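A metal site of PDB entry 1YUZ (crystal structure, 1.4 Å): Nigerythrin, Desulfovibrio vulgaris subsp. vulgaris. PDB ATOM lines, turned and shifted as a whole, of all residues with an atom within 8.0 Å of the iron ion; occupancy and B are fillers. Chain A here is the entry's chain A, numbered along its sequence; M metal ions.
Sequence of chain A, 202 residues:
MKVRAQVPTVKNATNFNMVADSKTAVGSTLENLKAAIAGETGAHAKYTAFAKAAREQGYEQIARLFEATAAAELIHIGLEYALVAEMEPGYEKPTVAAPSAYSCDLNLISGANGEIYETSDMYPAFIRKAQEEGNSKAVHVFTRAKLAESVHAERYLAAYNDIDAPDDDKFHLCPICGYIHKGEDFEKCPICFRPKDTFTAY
SG of Cys 192 sits close to N of Arg 194 (3.6 Å). The side-chain sulfur (SG) of Cys 177 sits close to the backbone NH (N) of Tyr 179 (3.4 Å). N of Cys 174 is in hydrogen-bond range of O of Tyr 179 (3.0 Å). The side-chain sulfur (SG) of Cys 174 lies close to the backbone NH (N) of Ile 176, 3.6 Å away. N of Ile 191 sits close to SG of Cys 189, at 3.4 Å. The backbone NH (N) of Cys 189 sits at hydrogen-bond distance from the backbone carbonyl oxygen (O) of Arg 194, at 2.8 Å.
The iron ion is bound by the side-chain sulfur (SG) of Cys 192 (2.2 Å), the side-chain sulfur (SG) of Cys 177 (2.3 Å), the side-chain sulfur (SG) of Cys 174 (2.3 Å) and the side-chain sulfur (SG) of Cys 189 (2.4 Å). The iron ion has four donor atoms within binding distance.
Of the 21 residues printed, 4 come within 4 Å of the iron ion.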
ATOM      1  N   ILE A  75       5.200  34.781  24.384  1.00  0.00           N
ATOM      2  CA  ILE A  75       4.454  33.862  25.233  1.00  0.00           C
ATOM      3  C   ILE A  75       5.453  32.881  25.842  1.00  0.00           C
ATOM      4  O   ILE A  75       5.391  32.577  27.033  1.00  0.00           O
ATOM      5  CB  ILE A  75       3.385  33.089  24.413  1.00  0.00           C
ATOM      6  CG1 ILE A  75       2.228  34.025  24.077  1.00  0.00           C
ATOM      7  CG2 ILE A  75       2.878  31.879  25.205  1.00  0.00           C
ATOM      8  CD1 ILE A  75       1.171  33.423  23.169  1.00  0.00           C
ATOM      9  N   ARG A 144       6.310  22.601  25.615  1.00  0.00           N
ATOM     10  CA  ARG A 144       5.321  23.441  24.954  1.00  0.00           C
ATOM     11  C   ARG A 144       6.005  24.360  23.940  1.00  0.00           C
ATOM     12  O   ARG A 144       5.544  24.510  22.812  1.00  0.00           O
ATOM     13  CB  ARG A 144       4.559  24.253  26.008  1.00  0.00           C
ATOM     14  CG  ARG A 144       3.398  25.060  25.470  1.00  0.00           C
ATOM     15  CD  ARG A 144       2.294  25.181  26.505  1.00  0.00           C
ATOM     16  NE  ARG A 144       1.624  23.895  26.718  1.00  0.00           N
ATOM     17  CZ  ARG A 144       0.553  23.717  27.474  1.00  0.00           C
ATOM     18  NH1 ARG A 144      -0.002  24.757  28.104  1.00  0.00           N
ATOM     19  NH2 ARG A 144       0.004  22.513  27.589  1.00  0.00           N
ATOM     20  N   ALA A 148       5.901  24.368  19.516  1.00  0.00           N
ATOM     21  CA  ALA A 148       5.508  25.521  18.733  1.00  0.00           C
ATOM     22  C   ALA A 148       6.568  25.901  17.709  1.00  0.00           C
ATOM     23  O   ALA A 148       6.245  26.314  16.599  1.00  0.00           O
ATOM     24  CB  ALA A 148       5.232  26.709  19.640  1.00  0.00           C
ATOM     25  N   LEU A 173      -3.075  33.000  16.780  1.00  0.00           N
ATOM     26  CA  LEU A 173      -2.115  32.625  17.807  1.00  0.00           C
ATOM     27  C   LEU A 173      -2.831  32.153  19.063  1.00  0.00           C
ATOM     28  O   LEU A 173      -3.761  32.801  19.539  1.00  0.00           O
ATOM     29  CB  LEU A 173      -1.221  33.819  18.143  1.00  0.00           C
ATOM     30  CG  LEU A 173      -0.232  33.610  19.295  1.00  0.00           C
ATOM     31  CD1 LEU A 173       0.788  32.534  18.919  1.00  0.00           C
ATOM     32  CD2 LEU A 173       0.473  34.927  19.590  1.00  0.00           C
ATOM     33  N   CYS A 174      -2.382  31.026  19.606  1.00  0.00           N
ATOM     34  CA  CYS A 174      -2.955  30.473  20.812  1.00  0.00           C
ATOM     35  C   CYS A 174      -2.722  31.418  21.986  1.00  0.00           C
ATOM     36  O   CYS A 174      -1.722  32.127  22.022  1.00  0.00           O
ATOM     37  CB  CYS A 174      -2.334  29.107  21.100  1.00  0.00           C
ATOM     38  SG  CYS A 174      -2.912  28.306  22.600  1.00  0.00           S
ATOM     39  N   PRO A 175      -3.640  31.454  22.948  1.00  0.00           N
ATOM     40  CA  PRO A 175      -3.477  32.347  24.097  1.00  0.00           C
ATOM     41  C   PRO A 175      -2.395  31.933  25.097  1.00  0.00           C
ATOM     42  O   PRO A 175      -1.798  32.785  25.743  1.00  0.00           O
ATOM     43  CB  PRO A 175      -4.869  32.335  24.739  1.00  0.00           C
ATOM     44  CG  PRO A 175      -5.350  30.956  24.444  1.00  0.00           C
ATOM     45  CD  PRO A 175      -4.953  30.786  22.992  1.00  0.00           C
ATOM     46  N   ILE A 176      -2.121  30.636  25.206  1.00  0.00           N
ATOM     47  CA  ILE A 176      -1.137  30.161  26.168  1.00  0.00           C
ATOM     48  C   ILE A 176       0.088  29.436  25.636  1.00  0.00           C
ATOM     49  O   ILE A 176       0.977  29.057  26.411  1.00  0.00           O
ATOM     50  CB  ILE A 176      -1.809  29.298  27.260  1.00  0.00           C
ATOM     51  CG1 ILE A 176      -2.392  28.032  26.639  1.00  0.00           C
ATOM     52  CG2 ILE A 176      -2.903  30.103  27.948  1.00  0.00           C
ATOM     53  CD1 ILE A 176      -2.943  27.054  27.658  1.00  0.00           C
ATOM     54  N   CYS A 177       0.151  29.202  24.332  1.00  0.00           N
ATOM     55  CA  CYS A 177       1.327  28.562  23.757  1.00  0.00           C
ATOM     56  C   CYS A 177       1.629  29.240  22.429  1.00  0.00           C
ATOM     57  O   CYS A 177       0.864  30.110  21.984  1.00  0.00           O
ATOM     58  CB  CYS A 177       1.138  27.047  23.603  1.00  0.00           C
ATOM     59  SG  CYS A 177       0.323  26.449  22.117  1.00  0.00           S
ATOM     60  N   GLY A 178       2.726  28.863  21.800  1.00  0.00           N
ATOM     61  CA  GLY A 178       3.117  29.500  20.560  1.00  0.00           C
ATOM     62  C   GLY A 178       2.485  29.002  19.286  1.00  0.00           C
ATOM     63  O   GLY A 178       2.871  29.428  18.194  1.00  0.00           O
ATOM     64  N   TYR A 179       1.496  28.122  19.386  1.00  0.00           N
ATOM     65  CA  TYR A 179       0.859  27.600  18.187  1.00  0.00           C
ATOM     66  C   TYR A 179       0.231  28.690  17.319  1.00  0.00           C
ATOM     67  O   TYR A 179      -0.473  29.558  17.815  1.00  0.00           O
ATOM     68  CB  TYR A 179      -0.207  26.577  18.538  1.00  0.00           C
ATOM     69  CG  TYR A 179      -0.873  25.996  17.312  1.00  0.00           C
ATOM     70  CD1 TYR A 179      -0.180  25.150  16.456  1.00  0.00           C
ATOM     71  CD2 TYR A 179      -2.196  26.323  17.001  1.00  0.00           C
ATOM     72  CE1 TYR A 179      -0.775  24.651  15.299  1.00  0.00           C
ATOM     73  CE2 TYR A 179      -2.801  25.816  15.856  1.00  0.00           C
ATOM     74  CZ  TYR A 179      -2.082  24.988  15.009  1.00  0.00           C
ATOM     75  OH  TYR A 179      -2.690  24.479  13.886  1.00  0.00           O
ATOM     76  N   ILE A 180       0.502  28.620  16.011  1.00  0.00           N
ATOM     77  CA  ILE A 180      -0.062  29.563  15.061  1.00  0.00           C
ATOM     78  C   ILE A 180      -0.738  28.787  13.944  1.00  0.00           C
ATOM     79  O   ILE A 180      -0.169  27.854  13.383  1.00  0.00           O
ATOM     80  CB  ILE A 180       1.039  30.461  14.428  1.00  0.00           C
ATOM     81  CG1 ILE A 180       1.637  31.372  15.498  1.00  0.00           C
ATOM     82  CG2 ILE A 180       0.447  31.294  13.276  1.00  0.00           C
ATOM     83  CD1 ILE A 180       2.876  32.109  15.042  1.00  0.00           C
ATOM     84  N   LYS A 188      -9.284  23.674  17.555  1.00  0.00           N
ATOM     85  CA  LYS A 188      -8.509  23.910  18.763  1.00  0.00           C
ATOM     86  C   LYS A 188      -7.018  23.767  18.530  1.00  0.00           C
ATOM     87  O   LYS A 188      -6.578  23.290  17.480  1.00  0.00           O
ATOM     88  CB  LYS A 188      -8.948  22.933  19.857  1.00  0.00           C
ATOM     89  CG  LYS A 188      -8.705  21.469  19.524  1.00  0.00           C
ATOM     90  CD  LYS A 188      -9.114  20.570  20.690  1.00  0.00           C
ATOM     91  CE  LYS A 188      -8.873  19.109  20.366  1.00  0.00           C
ATOM     92  NZ  LYS A 188      -9.270  18.219  21.498  1.00  0.00           N
ATOM     93  N   CYS A 189      -6.247  24.185  19.523  1.00  0.00           N
ATOM     94  CA  CYS A 189      -4.788  24.111  19.463  1.00  0.00           C
ATOM     95  C   CYS A 189      -4.318  22.661  19.593  1.00  0.00           C
ATOM     96  O   CYS A 189      -4.701  21.959  20.522  1.00  0.00           O
ATOM     97  CB  CYS A 189      -4.195  24.955  20.582  1.00  0.00           C
ATOM     98  SG  CYS A 189      -2.403  24.965  20.605  1.00  0.00           S
ATOM     99  N   PRO A 190      -3.485  22.199  18.654  1.00  0.00           N
ATOM    100  CA  PRO A 190      -2.988  20.822  18.716  1.00  0.00           C
ATOM    101  C   PRO A 190      -1.918  20.609  19.786  1.00  0.00           C
ATOM    102  O   PRO A 190      -1.573  19.474  20.105  1.00  0.00           O
ATOM    103  CB  PRO A 190      -2.445  20.591  17.314  1.00  0.00           C
ATOM    104  CG  PRO A 190      -1.900  21.933  16.958  1.00  0.00           C
ATOM    105  CD  PRO A 190      -3.010  22.864  17.429  1.00  0.00           C
ATOM    106  N   ILE A 191      -1.413  21.711  20.348  1.00  0.00           N
ATOM    107  CA  ILE A 191      -0.389  21.620  21.383  1.00  0.00           C
ATOM    108  C   ILE A 191      -0.979  21.632  22.797  1.00  0.00           C
ATOM    109  O   ILE A 191      -0.578  20.828  23.629  1.00  0.00           O
ATOM    110  CB  ILE A 191       0.628  22.784  21.251  1.00  0.00           C
ATOM    111  CG1 ILE A 191       1.424  22.623  19.945  1.00  0.00           C
ATOM    112  CG2 ILE A 191       1.573  22.800  22.458  1.00  0.00           C
ATOM    113  CD1 ILE A 191       2.401  23.757  19.676  1.00  0.00           C
ATOM    114  N   CYS A 192      -1.925  22.534  23.049  1.00  0.00           N
ATOM    115  CA  CYS A 192      -2.509  22.625  24.389  1.00  0.00           C
ATOM    116  C   CYS A 192      -4.034  22.439  24.420  1.00  0.00           C
ATOM    117  O   CYS A 192      -4.629  22.483  25.493  1.00  0.00           O
ATOM    118  CB  CYS A 192      -2.155  23.968  25.024  1.00  0.00           C
ATOM    119  SG  CYS A 192      -2.979  25.368  24.248  1.00  0.00           S
ATOM    120  N   PHE A 193      -4.639  22.252  23.257  1.00  0.00           N
ATOM    121  CA  PHE A 193      -6.081  22.040  23.149  1.00  0.00           C
ATOM    122  C   PHE A 193      -6.991  23.240  23.376  1.00  0.00           C
ATOM    123  O   PHE A 193      -8.217  23.092  23.414  1.00  0.00           O
ATOM    124  CB  PHE A 193      -6.510  20.884  24.075  1.00  0.00           C
ATOM    125  CG  PHE A 193      -6.206  19.519  23.517  1.00  0.00           C
ATOM    126  CD1 PHE A 193      -5.308  19.349  22.474  1.00  0.00           C
ATOM    127  CD2 PHE A 193      -6.829  18.387  24.059  1.00  0.00           C
ATOM    128  CE1 PHE A 193      -5.016  18.073  21.977  1.00  0.00           C
ATOM    129  CE2 PHE A 193      -6.538  17.115  23.571  1.00  0.00           C
ATOM    130  CZ  PHE A 193      -5.631  16.955  22.526  1.00  0.00           C
ATOM    131  N   ARG A 194      -6.422  24.430  23.533  1.00  0.00           N
ATOM    132  CA  ARG A 194      -7.246  25.625  23.723  1.00  0.00           C
ATOM    133  C   ARG A 194      -8.159  25.802  22.499  1.00  0.00           C
ATOM    134  O   ARG A 194      -7.716  25.672  21.366  1.00  0.00           O
ATOM    135  CB  ARG A 194      -6.370  26.867  23.894  1.00  0.00           C
ATOM    136  CG  ARG A 194      -5.991  27.174  25.328  1.00  0.00           C
ATOM    137  CD  ARG A 194      -7.191  27.682  26.115  1.00  0.00           C
ATOM    138  NE  ARG A 194      -6.847  28.143  27.459  1.00  0.00           N
ATOM    139  CZ  ARG A 194      -6.601  27.336  28.481  1.00  0.00           C
ATOM    140  NH1 ARG A 194      -6.680  26.012  28.338  1.00  0.00           N
ATOM    141  NH2 ARG A 194      -6.287  27.848  29.668  1.00  0.00           N
ATOM    142  N   PRO A 195      -9.441  26.100  22.732  1.00  0.00           N
ATOM    143  CA  PRO A 195     -10.394  26.303  21.633  1.00  0.00           C
ATOM    144  C   PRO A 195     -10.063  27.514  20.764  1.00  0.00           C
ATOM    145  O   PRO A 195      -9.508  28.498  21.241  1.00  0.00           O
ATOM    146  CB  PRO A 195     -11.740  26.448  22.351  1.00  0.00           C
ATOM    147  CG  PRO A 195     -11.537  25.662  23.619  1.00  0.00           C
ATOM    148  CD  PRO A 195     -10.146  26.091  24.024  1.00  0.00           C
ATOM    149  N   THR A 198     -10.435  31.276  21.721  1.00  0.00           N
ATOM    150  CA  THR A 198      -9.536  31.953  22.646  1.00  0.00           C
ATOM    151  C   THR A 198      -8.290  32.507  21.958  1.00  0.00           C
ATOM    152  O   THR A 198      -7.466  33.172  22.590  1.00  0.00           O
ATOM    153  CB  THR A 198      -9.087  31.009  23.782  1.00  0.00           C
ATOM    154  OG1 THR A 198      -8.329  29.918  23.233  1.00  0.00           O
ATOM    155  CG2 THR A 198     -10.298  30.458  24.519  1.00  0.00           C
ATOM    156  N   PHE A 199      -8.148  32.212  20.671  1.00  0.00           N
ATOM    157  CA  PHE A 199      -6.996  32.670  19.884  1.00  0.00           C
ATOM    158  C   PHE A 199      -7.088  34.151  19.540  1.00  0.00           C
ATOM    159  O   PHE A 199      -8.173  34.751  19.580  1.00  0.00           O
ATOM    160  CB  PHE A 199      -6.891  31.874  18.582  1.00  0.00           C
ATOM    161  CG  PHE A 199      -6.266  30.517  18.736  1.00  0.00           C
ATOM    162  CD1 PHE A 199      -6.755  29.596  19.667  1.00  0.00           C
ATOM    163  CD2 PHE A 199      -5.188  30.149  17.925  1.00  0.00           C
ATOM    164  CE1 PHE A 199      -6.190  28.332  19.773  1.00  0.00           C
ATOM    165  CE2 PHE A 199      -4.624  28.885  18.031  1.00  0.00           C
ATOM    166  CZ  PHE A 199      -5.114  27.973  18.958  1.00  0.00           C
HETATM  167 FE    FE M   1      -1.906  26.248  22.514  1.00  0.00          FE
